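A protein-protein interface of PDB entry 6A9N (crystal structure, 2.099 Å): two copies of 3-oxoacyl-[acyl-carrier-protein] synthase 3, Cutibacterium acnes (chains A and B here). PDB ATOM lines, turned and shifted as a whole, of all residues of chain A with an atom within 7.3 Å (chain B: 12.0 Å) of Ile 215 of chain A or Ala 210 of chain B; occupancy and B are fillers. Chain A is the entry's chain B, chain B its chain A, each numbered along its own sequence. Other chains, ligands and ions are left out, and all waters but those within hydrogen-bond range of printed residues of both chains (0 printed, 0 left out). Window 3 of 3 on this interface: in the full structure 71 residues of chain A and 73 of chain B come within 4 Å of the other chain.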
ATOM      1  N   GLU A 155      17.220 -31.365  25.058  1.00  0.00           N
ATOM      2  CA  GLU A 155      17.065 -29.959  24.685  1.00  0.00           C
ATOM      3  C   GLU A 155      18.362 -29.348  24.156  1.00  0.00           C
ATOM      4  O   GLU A 155      18.307 -28.377  23.397  1.00  0.00           O
ATOM      5  CB  GLU A 155      16.582 -29.131  25.877  1.00  0.00           C
ATOM      6  CG  GLU A 155      15.167 -29.410  26.345  1.00  0.00           C
ATOM      7  CD  GLU A 155      14.846 -28.731  27.672  1.00  0.00           C
ATOM      8  OE1 GLU A 155      13.661 -28.396  27.902  1.00  0.00           O
ATOM      9  OE2 GLU A 155      15.779 -28.540  28.495  1.00  0.00           O
ATOM     10  N   TRP A 205      24.836 -19.730  27.122  1.00  0.00           N
ATOM     11  CA  TRP A 205      23.455 -19.277  27.001  1.00  0.00           C
ATOM     12  C   TRP A 205      23.303 -17.928  26.298  1.00  0.00           C
ATOM     13  O   TRP A 205      22.361 -17.797  25.498  1.00  0.00           O
ATOM     14  CB  TRP A 205      22.792 -19.250  28.389  1.00  0.00           C
ATOM     15  CG  TRP A 205      21.973 -20.467  28.680  1.00  0.00           C
ATOM     16  CD1 TRP A 205      22.254 -21.454  29.586  1.00  0.00           C
ATOM     17  CD2 TRP A 205      20.724 -20.824  28.072  1.00  0.00           C
ATOM     18  NE1 TRP A 205      21.250 -22.403  29.583  1.00  0.00           N
ATOM     19  CE2 TRP A 205      20.305 -22.043  28.656  1.00  0.00           C
ATOM     20  CE3 TRP A 205      19.924 -20.237  27.084  1.00  0.00           C
ATOM     21  CZ2 TRP A 205      19.123 -22.686  28.282  1.00  0.00           C
ATOM     22  CZ3 TRP A 205      18.745 -20.879  26.717  1.00  0.00           C
ATOM     23  CH2 TRP A 205      18.360 -22.087  27.310  1.00  0.00           C
ATOM     24  N   THR A 207      24.923 -16.698  23.823  1.00  0.00           N
ATOM     25  CA  THR A 207      25.002 -17.016  22.403  1.00  0.00           C
ATOM     26  C   THR A 207      23.693 -17.610  21.904  1.00  0.00           C
ATOM     27  O   THR A 207      23.183 -17.227  20.845  1.00  0.00           O
ATOM     28  CB  THR A 207      26.160 -17.990  22.160  1.00  0.00           C
ATOM     29  OG1 THR A 207      27.386 -17.367  22.548  1.00  0.00           O
ATOM     30  CG2 THR A 207      26.257 -18.367  20.694  1.00  0.00           C
ATOM     31  N   ALA A 208      23.136 -18.560  22.656  1.00  0.00           N
ATOM     32  CA  ALA A 208      21.868 -19.157  22.256  1.00  0.00           C
ATOM     33  C   ALA A 208      20.747 -18.129  22.313  1.00  0.00           C
ATOM     34  O   ALA A 208      19.880 -18.096  21.428  1.00  0.00           O
ATOM     35  CB  ALA A 208      21.549 -20.358  23.146  1.00  0.00           C
ATOM     36  N   SER A 209      20.768 -17.259  23.327  1.00  0.00           N
ATOM     37  CA  SER A 209      19.693 -16.280  23.478  1.00  0.00           C
ATOM     38  C   SER A 209      19.671 -15.291  22.319  1.00  0.00           C
ATOM     39  O   SER A 209      18.596 -14.921  21.828  1.00  0.00           O
ATOM     40  CB  SER A 209      19.840 -15.540  24.804  1.00  0.00           C
ATOM     41  OG  SER A 209      18.740 -14.662  25.020  1.00  0.00           O
ATOM     42  N   ALA A 210      20.851 -14.852  21.875  1.00  0.00           N
ATOM     43  CA  ALA A 210      20.965 -13.900  20.777  1.00  0.00           C
ATOM     44  C   ALA A 210      20.525 -14.513  19.449  1.00  0.00           C
ATOM     45  O   ALA A 210      20.117 -13.784  18.541  1.00  0.00           O
ATOM     46  CB  ALA A 210      22.414 -13.399  20.675  1.00  0.00           C
ATOM     47  N   ASP A 211      20.604 -15.834  19.316  1.00  0.00           N
ATOM     48  CA  ASP A 211      20.326 -16.529  18.059  1.00  0.00           C
ATOM     49  C   ASP A 211      18.824 -16.602  17.823  1.00  0.00           C
ATOM     50  O   ASP A 211      18.119 -17.292  18.567  1.00  0.00           O
ATOM     51  CB  ASP A 211      20.921 -17.941  18.081  1.00  0.00           C
ATOM     52  CG  ASP A 211      20.958 -18.593  16.704  1.00  0.00           C
ATOM     53  OD1 ASP A 211      20.012 -18.417  15.913  1.00  0.00           O
ATOM     54  OD2 ASP A 211      21.940 -19.290  16.413  1.00  0.00           O
ATOM     55  N   PRO A 212      18.297 -15.916  16.806  1.00  0.00           N
ATOM     56  CA  PRO A 212      16.845 -15.957  16.569  1.00  0.00           C
ATOM     57  C   PRO A 212      16.297 -17.338  16.240  1.00  0.00           C
ATOM     58  O   PRO A 212      15.086 -17.543  16.367  1.00  0.00           O
ATOM     59  CB  PRO A 212      16.657 -15.003  15.380  1.00  0.00           C
ATOM     60  CG  PRO A 212      17.989 -15.005  14.691  1.00  0.00           C
ATOM     61  CD  PRO A 212      18.998 -15.099  15.797  1.00  0.00           C
ATOM     62  N   ASN A 213      17.124 -18.288  15.800  1.00  0.00           N
ATOM     63  CA  ASN A 213      16.610 -19.591  15.383  1.00  0.00           C
ATOM     64  C   ASN A 213      16.922 -20.699  16.383  1.00  0.00           C
ATOM     65  O   ASN A 213      16.951 -21.876  16.013  1.00  0.00           O
ATOM     66  CB  ASN A 213      17.153 -19.954  14.002  1.00  0.00           C
ATOM     67  CG  ASN A 213      16.717 -18.967  12.941  1.00  0.00           C
ATOM     68  OD1 ASN A 213      15.534 -18.661  12.815  1.00  0.00           O
ATOM     69  ND2 ASN A 213      17.677 -18.437  12.195  1.00  0.00           N
ATOM     70  N   LYS A 214      17.141 -20.355  17.647  1.00  0.00           N
ATOM     71  CA  LYS A 214      17.575 -21.347  18.617  1.00  0.00           C
ATOM     72  C   LYS A 214      17.000 -20.963  19.968  1.00  0.00           C
ATOM     73  O   LYS A 214      16.868 -19.776  20.263  1.00  0.00           O
ATOM     74  CB  LYS A 214      19.109 -21.405  18.635  1.00  0.00           C
ATOM     75  CG  LYS A 214      19.725 -22.332  19.639  1.00  0.00           C
ATOM     76  CD  LYS A 214      21.249 -22.150  19.685  1.00  0.00           C
ATOM     77  CE  LYS A 214      21.931 -22.905  18.560  1.00  0.00           C
ATOM     78  NZ  LYS A 214      23.397 -22.602  18.481  1.00  0.00           N
ATOM     79  N   ILE A 215      16.626 -21.954  20.779  1.00  0.00           N
ATOM     80  CA  ILE A 215      16.295 -21.652  22.172  1.00  0.00           C
ATOM     81  C   ILE A 215      17.494 -21.983  23.055  1.00  0.00           C
ATOM     82  O   ILE A 215      18.046 -21.098  23.718  1.00  0.00           O
ATOM     83  CB  ILE A 215      15.034 -22.387  22.666  1.00  0.00           C
ATOM     84  CG1 ILE A 215      13.792 -21.906  21.906  1.00  0.00           C
ATOM     85  CG2 ILE A 215      14.816 -22.099  24.158  1.00  0.00           C
ATOM     86  CD1 ILE A 215      13.615 -20.388  21.939  1.00  0.00           C
ATOM     87  N   HIS A 216      17.938 -23.307  23.059  1.00  0.00           N
ATOM     88  CA  HIS A 216      18.914 -23.853  23.984  1.00  0.00           C
ATOM     89  C   HIS A 216      20.318 -23.875  23.388  1.00  0.00           C
ATOM     90  O   HIS A 216      20.489 -24.065  22.184  1.00  0.00           O
ATOM     91  CB  HIS A 216      18.526 -25.279  24.385  1.00  0.00           C
ATOM     92  CG  HIS A 216      17.285 -25.356  25.209  1.00  0.00           C
ATOM     93  ND1 HIS A 216      16.024 -25.410  24.654  1.00  0.00           N
ATOM     94  CD2 HIS A 216      17.106 -25.379  26.554  1.00  0.00           C
ATOM     95  CE1 HIS A 216      15.123 -25.469  25.619  1.00  0.00           C
ATOM     96  NE2 HIS A 216      15.752 -25.450  26.781  1.00  0.00           N
ATOM     97  N   PRO A 217      21.358 -23.708  24.208  1.00  0.00           N
ATOM     98  CA  PRO A 217      22.715 -23.970  23.720  1.00  0.00           C
ATOM     99  C   PRO A 217      22.877 -25.444  23.380  1.00  0.00           C
ATOM    100  O   PRO A 217      22.106 -26.299  23.820  1.00  0.00           O
ATOM    101  CB  PRO A 217      23.604 -23.564  24.899  1.00  0.00           C
ATOM    102  CG  PRO A 217      22.749 -23.756  26.088  1.00  0.00           C
ATOM    103  CD  PRO A 217      21.330 -23.458  25.657  1.00  0.00           C
ATOM    104  N   HIS B  95      26.944 -18.705  32.779  1.00  0.00           N
ATOM    105  CA  HIS B  95      25.781 -18.970  31.942  1.00  0.00           C
ATOM    106  C   HIS B  95      26.046 -20.027  30.887  1.00  0.00           C
ATOM    107  O   HIS B  95      25.284 -20.140  29.923  1.00  0.00           O
ATOM    108  CB  HIS B  95      25.279 -17.669  31.306  1.00  0.00           C
ATOM    109  CG  HIS B  95      24.882 -16.625  32.310  1.00  0.00           C
ATOM    110  ND1 HIS B  95      24.007 -16.881  33.345  1.00  0.00           N
ATOM    111  CD2 HIS B  95      25.255 -15.330  32.445  1.00  0.00           C
ATOM    112  CE1 HIS B  95      23.849 -15.785  34.068  1.00  0.00           C
ATOM    113  NE2 HIS B  95      24.597 -14.829  33.543  1.00  0.00           N
ATOM    114  N   ARG B  96      27.062 -20.796  31.044  1.00  0.00           N
ATOM    115  CA  ARG B  96      27.298 -21.938  30.184  1.00  0.00           C
ATOM    116  C   ARG B  96      26.940 -23.201  30.943  1.00  0.00           C
ATOM    117  O   ARG B  96      27.390 -23.353  32.084  1.00  0.00           O
ATOM    118  CB  ARG B  96      28.760 -21.979  29.758  1.00  0.00           C
ATOM    119  CG  ARG B  96      29.045 -22.975  28.658  1.00  0.00           C
ATOM    120  CD  ARG B  96      30.540 -23.103  28.423  1.00  0.00           C
ATOM    121  NE  ARG B  96      31.184 -21.823  28.098  1.00  0.00           N
ATOM    122  CZ  ARG B  96      31.331 -21.353  26.861  1.00  0.00           C
ATOM    123  NH1 ARG B  96      30.863 -22.043  25.821  1.00  0.00           N
ATOM    124  NH2 ARG B  96      31.931 -20.182  26.659  1.00  0.00           N
ATOM    125  N   PRO B  97      26.132 -24.117  30.393  1.00  0.00           N
ATOM    126  CA  PRO B  97      25.777 -25.314  31.178  1.00  0.00           C
ATOM    127  C   PRO B  97      26.980 -26.139  31.596  1.00  0.00           C
ATOM    128  O   PRO B  97      27.034 -26.626  32.732  1.00  0.00           O
ATOM    129  CB  PRO B  97      24.852 -26.097  30.231  1.00  0.00           C
ATOM    130  CG  PRO B  97      24.250 -25.041  29.340  1.00  0.00           C
ATOM    131  CD  PRO B  97      25.373 -24.032  29.133  1.00  0.00           C
ATOM    132  N   GLU B 203      14.485 -14.982  36.168  1.00  0.00           N
ATOM    133  CA  GLU B 203      13.810 -15.567  35.018  1.00  0.00           C
ATOM    134  C   GLU B 203      14.605 -16.760  34.509  1.00  0.00           C
ATOM    135  O   GLU B 203      15.814 -16.867  34.720  1.00  0.00           O
ATOM    136  CB  GLU B 203      13.648 -14.538  33.899  1.00  0.00           C
ATOM    137  CG  GLU B 203      12.821 -13.340  34.304  1.00  0.00           C
ATOM    138  CD  GLU B 203      12.774 -12.281  33.221  1.00  0.00           C
ATOM    139  OE1 GLU B 203      13.842 -11.953  32.644  1.00  0.00           O
ATOM    140  OE2 GLU B 203      11.664 -11.782  32.951  1.00  0.00           O
ATOM    141  N   ASP B 204      13.922 -17.667  33.829  1.00  0.00           N
ATOM    142  CA  ASP B 204      14.635 -18.809  33.279  1.00  0.00           C
ATOM    143  C   ASP B 204      15.247 -18.434  31.936  1.00  0.00           C
ATOM    144  O   ASP B 204      14.741 -17.565  31.214  1.00  0.00           O
ATOM    145  CB  ASP B 204      13.707 -20.017  33.128  1.00  0.00           C
ATOM    146  CG  ASP B 204      12.508 -19.704  32.286  1.00  0.00           C
ATOM    147  OD1 ASP B 204      12.497 -20.099  31.104  1.00  0.00           O
ATOM    148  OD2 ASP B 204      11.584 -19.024  32.789  1.00  0.00           O
ATOM    149  N   TRP B 205      16.357 -19.088  31.613  1.00  0.00           N
ATOM    150  CA  TRP B 205      17.036 -18.794  30.357  1.00  0.00           C
ATOM    151  C   TRP B 205      16.196 -19.082  29.116  1.00  0.00           C
ATOM    152  O   TRP B 205      16.279 -18.281  28.169  1.00  0.00           O
ATOM    153  CB  TRP B 205      18.360 -19.552  30.298  1.00  0.00           C
ATOM    154  CG  TRP B 205      19.532 -18.736  30.778  1.00  0.00           C
ATOM    155  CD1 TRP B 205      20.226 -18.898  31.952  1.00  0.00           C
ATOM    156  CD2 TRP B 205      20.147 -17.639  30.097  1.00  0.00           C
ATOM    157  NE1 TRP B 205      21.231 -17.959  32.039  1.00  0.00           N
ATOM    158  CE2 TRP B 205      21.210 -17.179  30.913  1.00  0.00           C
ATOM    159  CE3 TRP B 205      19.909 -16.996  28.876  1.00  0.00           C
ATOM    160  CZ2 TRP B 205      22.031 -16.113  30.541  1.00  0.00           C
ATOM    161  CZ3 TRP B 205      20.729 -15.921  28.519  1.00  0.00           C
ATOM    162  CH2 TRP B 205      21.769 -15.495  29.349  1.00  0.00           C
ATOM    163  N   PRO B 206      15.410 -20.182  29.020  1.00  0.00           N
ATOM    164  CA  PRO B 206      14.600 -20.381  27.799  1.00  0.00           C
ATOM    165  C   PRO B 206      13.609 -19.257  27.538  1.00  0.00           C
ATOM    166  O   PRO B 206      13.359 -18.912  26.377  1.00  0.00           O
ATOM    167  CB  PRO B 206      13.885 -21.719  28.065  1.00  0.00           C
ATOM    168  CG  PRO B 206      14.830 -22.449  28.950  1.00  0.00           C
ATOM    169  CD  PRO B 206      15.392 -21.390  29.870  1.00  0.00           C
ATOM    170  N   THR B 207      13.039 -18.677  28.592  1.00  0.00           N
ATOM    171  CA  THR B 207      12.170 -17.519  28.438  1.00  0.00           C
ATOM    172  C   THR B 207      12.946 -16.314  27.914  1.00  0.00           C
ATOM    173  O   THR B 207      12.523 -15.663  26.951  1.00  0.00           O
ATOM    174  CB  THR B 207      11.512 -17.201  29.776  1.00  0.00           C
ATOM    175  OG1 THR B 207      10.673 -18.290  30.134  1.00  0.00           O
ATOM    176  CG2 THR B 207      10.683 -15.918  29.712  1.00  0.00           C
ATOM    177  N   ALA B 208      14.092 -16.004  28.533  1.00  0.00           N
ATOM    178  CA  ALA B 208      14.927 -14.929  28.012  1.00  0.00           C
ATOM    179  C   ALA B 208      15.343 -15.206  26.570  1.00  0.00           C
ATOM    180  O   ALA B 208      15.397 -14.288  25.739  1.00  0.00           O
ATOM    181  CB  ALA B 208      16.161 -14.738  28.893  1.00  0.00           C
ATOM    182  N   SER B 209      15.629 -16.469  26.252  1.00  0.00           N
ATOM    183  CA  SER B 209      16.159 -16.786  24.933  1.00  0.00           C
ATOM    184  C   SER B 209      15.121 -16.551  23.844  1.00  0.00           C
ATOM    185  O   SER B 209      15.469 -16.120  22.736  1.00  0.00           O
ATOM    186  CB  SER B 209      16.652 -18.229  24.896  1.00  0.00           C
ATOM    187  OG  SER B 209      17.217 -18.517  23.624  1.00  0.00           O
ATOM    188  N   ALA B 210      13.844 -16.837  24.135  1.00  0.00           N
ATOM    189  CA  ALA B 210      12.777 -16.634  23.161  1.00  0.00           C
ATOM    190  C   ALA B 210      12.413 -15.162  22.991  1.00  0.00           C
ATOM    191  O   ALA B 210      11.822 -14.799  21.969  1.00  0.00           O
ATOM    192  CB  ALA B 210      11.526 -17.431  23.564  1.00  0.00           C
ATOM    193  N   ASP B 211      12.755 -14.314  23.954  1.00  0.00           N
ATOM    194  CA  ASP B 211      12.398 -12.904  23.887  1.00  0.00           C
ATOM    195  C   ASP B 211      13.355 -12.156  22.958  1.00  0.00           C
ATOM    196  O   ASP B 211      14.554 -12.085  23.251  1.00  0.00           O
ATOM    197  CB  ASP B 211      12.430 -12.305  25.280  1.00  0.00           C
ATOM    198  CG  ASP B 211      11.807 -10.921  25.336  1.00  0.00           C
ATOM    199  OD1 ASP B 211      11.933 -10.161  24.349  1.00  0.00           O
ATOM    200  OD2 ASP B 211      11.201 -10.597  26.379  1.00  0.00           O
ATOM    201  N   PRO B 212      12.867 -11.547  21.867  1.00  0.00           N
ATOM    202  CA  PRO B 212      13.776 -10.858  20.935  1.00  0.00           C
ATOM    203  C   PRO B 212      14.306  -9.535  21.464  1.00  0.00           C
ATOM    204  O   PRO B 212      15.209  -8.953  20.840  1.00  0.00           O
ATOM    205  CB  PRO B 212      12.897 -10.638  19.700  1.00  0.00           C
ATOM    206  CG  PRO B 212      11.522 -10.438  20.294  1.00  0.00           C
ATOM    207  CD  PRO B 212      11.459 -11.443  21.436  1.00  0.00           C
ATOM    208  N   ASN B 213      13.783  -9.048  22.582  1.00  0.00           N
ATOM    209  CA  ASN B 213      14.185  -7.771  23.150  1.00  0.00           C
ATOM    210  C   ASN B 213      15.224  -7.887  24.264  1.00  0.00           C
ATOM    211  O   ASN B 213      15.650  -6.856  24.793  1.00  0.00           O
ATOM    212  CB  ASN B 213      12.958  -7.027  23.691  1.00  0.00           C
ATOM    213  CG  ASN B 213      12.041  -6.523  22.592  1.00  0.00           C
ATOM    214  OD1 ASN B 213      10.830  -6.679  22.675  1.00  0.00           O
ATOM    215  ND2 ASN B 213      12.610  -5.923  21.558  1.00  0.00           N
ATOM    216  N   LYS B 214      15.650  -9.094  24.647  1.00  0.00           N
ATOM    217  CA  LYS B 214      16.622  -9.210  25.730  1.00  0.00           C
ATOM    218  C   LYS B 214      17.581 -10.357  25.452  1.00  0.00           C
ATOM    219  O   LYS B 214      17.298 -11.251  24.655  1.00  0.00           O
ATOM    220  CB  LYS B 214      15.933  -9.417  27.091  1.00  0.00           C
ATOM    221  CG  LYS B 214      15.295 -10.767  27.248  1.00  0.00           C
ATOM    222  CD  LYS B 214      14.073 -10.716  28.157  1.00  0.00           C
ATOM    223  CE  LYS B 214      14.451 -10.614  29.612  1.00  0.00           C
ATOM    224  NZ  LYS B 214      13.221 -10.648  30.456  1.00  0.00           N
ATOM    225  N   ILE B 215      18.738 -10.308  26.110  1.00  0.00           N
ATOM    226  CA  ILE B 215      19.677 -11.424  26.094  1.00  0.00           C
ATOM    227  C   ILE B 215      19.517 -12.210  27.394  1.00  0.00           C
ATOM    228  O   ILE B 215      19.193 -13.404  27.371  1.00  0.00           O
ATOM    229  CB  ILE B 215      21.126 -10.948  25.897  1.00  0.00           C
ATOM    230  CG1 ILE B 215      21.297 -10.285  24.522  1.00  0.00           C
ATOM    231  CG2 ILE B 215      22.105 -12.114  26.063  1.00  0.00           C
ATOM    232  CD1 ILE B 215      20.942 -11.195  23.328  1.00  0.00           C
ATOM    233  N   HIS B 216      19.712 -11.532  28.555  1.00  0.00           N
ATOM    234  CA  HIS B 216      19.825 -12.193  29.851  1.00  0.00           C
ATOM    235  C   HIS B 216      18.496 -12.223  30.594  1.00  0.00           C
ATOM    236  O   HIS B 216      17.655 -11.337  30.421  1.00  0.00           O
ATOM    237  CB  HIS B 216      20.858 -11.483  30.740  1.00  0.00           C
ATOM    238  CG  HIS B 216      22.263 -11.633  30.267  1.00  0.00           C
ATOM    239  ND1 HIS B 216      22.828 -10.788  29.336  1.00  0.00           N
ATOM    240  CD2 HIS B 216      23.216 -12.544  30.578  1.00  0.00           C
ATOM    241  CE1 HIS B 216      24.072 -11.166  29.099  1.00  0.00           C
ATOM    242  NE2 HIS B 216      24.332 -12.228  29.841  1.00  0.00           N
ATOM    243  N   PRO B 217      18.306 -13.245  31.430  1.00  0.00           N
ATOM    244  CA  PRO B 217      17.189 -13.241  32.379  1.00  0.00           C
ATOM    245  C   PRO B 217      17.401 -12.200  33.466  1.00  0.00           C
ATOM    246  O   PRO B 217      18.526 -11.816  33.779  1.00  0.00           O
ATOM    247  CB  PRO B 217      17.223 -14.655  32.970  1.00  0.00           C
ATOM    248  CG  PRO B 217      18.643 -15.069  32.843  1.00  0.00           C
ATOM    249  CD  PRO B 217      19.099 -14.481  31.521  1.00  0.00           C
ATOM    250  N   LEU B 218      16.298 -11.765  34.067  1.00  0.00           N
ATOM    251  CA  LEU B 218      16.331 -10.676  35.027  1.00  0.00           C
ATOM    252  C   LEU B 218      16.077 -11.174  36.443  1.00  0.00           C
ATOM    253  O   LEU B 218      15.391 -12.175  36.653  1.00  0.00           O
ATOM    254  CB  LEU B 218      15.302  -9.603  34.667  1.00  0.00           C
ATOM    255  CG  LEU B 218      15.550  -8.992  33.288  1.00  0.00           C
ATOM    256  CD1 LEU B 218      14.479  -7.988  32.966  1.00  0.00           C
ATOM    257  CD2 LEU B 218      16.948  -8.355  33.190  1.00  0.00           C
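Hydrophobic or aromatic side chains of chain A within 4 Å of the printed part of chain B: Trp 205, Ala 210, Ile 215, His 216 and Pro 217.
Hydrophobic or aromatic side chains of chain B that line the printed part of chain A: Pro 97, Trp 205, Pro 206, Ala 210 and Ile 215.
Among the printed residues, no Asp or Glu carboxylate lies within 4 Å of a Lys or Arg side-chain nitrogen of the other chain.
The backbone carbonyl oxygen of His 95 of chain B lies within hydrogen-bond range of the backbone NH of Trp 205 of chain A, at 2.9 Å.
O of Ala 208 of chain B is in hydrogen-bond range of OG of Ser 209 of chain A.
O of Ala 208 of chain A sits at hydrogen-bond distance from OG of Ser 209 of chain B, 3.5 Å away.
The side-chain hydroxyl (OG) of Ser 209 of chain B is in hydrogen-bond range of the backbone carbonyl oxygen (O) of Ile 215 of chain A, at 2.7 Å.
The backbone carbonyl oxygen (O) of Ile 215 of chain B lies within hydrogen-bond range of the side-chain hydroxyl (OG) of Ser 209 of chain A (2.7 Å).
The backbone carbonyl oxygen (O) of Ser 209 of chain A lies close to the backbone carbonyl oxygen (O) of Ser 209 of chain B, 3.5 Å away.
Of the printed residues of chain B, Trp 205 of chain A touches His 95 (2.9 Å), Trp 205 (3.5 Å), Pro 206 (3.9 Å) and Ser 209 (3.8 Å).
Ser 209 of chain A touches just these residues of chain B: Trp 205, Ala 208, Ser 209, Lys 214 and Ile 215.
Of the printed residues of chain B, Ala 210 of chain A touches Ile 215.
No residue of chain B comes within 4 Å of Asp 211 of chain A.
Lys 214 of chain A touches just one residue of chain B: Ser 209 (3.6 Å).
Of the printed residues of chain B, Ile 215 of chain A touches Ser 209 and Ala 210.
Pro 217 of chain A touches just one residue of chain B: Pro 97 (3.8 Å).
Printed residues of chain A within 4 Å of Trp 205 of chain B: Trp 205 and Ser 209.
Ser 209 of chain B touches just these residues of chain A: Trp 205, Ala 208, Ser 209, Lys 214 and Ile 215.
Ala 210 of chain B touches just one residue of chain A: Ile 215 (3.97 Å).
The nearest residue of chain A that does not touch Ala 210 of chain B is Ser 209 of chain A (5.4 Å).
The nearest printed residue of chain A that does not touch Pro 97 of chain B is Trp 205 of chain A (4.002 Å).
The indole nitrogen (NE1) of Trp 205 of chain B is in hydrogen-bond range of a ring nitrogen (ND1) of His 95 of chain B (3.3 Å).
The side-chain carboxylate of Glu 203 of chain B lies within salt-bridge range of the side-chain amino group of Lys 214 of chain B, 2.6 Å away.
Trp 205 of chain A touches Trp 205 of chain B.
CH2 of Trp 205 of chain A touches N of Pro 206 of chain B (3.9 Å).
Trp 205 of chain A touches Ser 209 of chain B (CZ3 to CB, 3.8 Å).
CZ3 of Trp 205 of chain B touches CB of Ser 209 of chain A, at 3.8 Å.
O of Lys 214 of chain B touches OG of Ser 209 of chain A (3.7 Å).
Ala 210 of chain A touches Ile 215 of chain B.
Lys 214 of chain A touches Ser 209 of chain B.
CB of Ala 210 of chain B touches CD1 of Ile 215 of chain A, at 3.97 Å.
CG of Pro 206 of chain B touches NE2 of His 216 of chain A, at 3.8 Å.
Pro 217 of chain A touches Pro 97 of chain B (CG to CG, 3.8 Å).
Trp 205 of chain A touches its own counterpart, Trp 205 of chain B.
Ala 208 of chain A touches Ser 209 of chain B, and with the chains exchanged Ser 209 of chain A touches Ala 208 of chain B.
Ser 209 of chain B touches its own counterpart, Ser 209 of chain A.
Ser 209 of chain A touches Lys 214 of chain B, and with the chains exchanged Lys 214 of chain A touches Ser 209 of chain B.
Positions printed for both chains: 205, 207, 208, 209, 210, 211, 212, 213, 214, 215, 216 and 217.
Of the 16 pairs that touch across the chains among the printed residues, 12 have their exchanged pair printed and touching as well.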
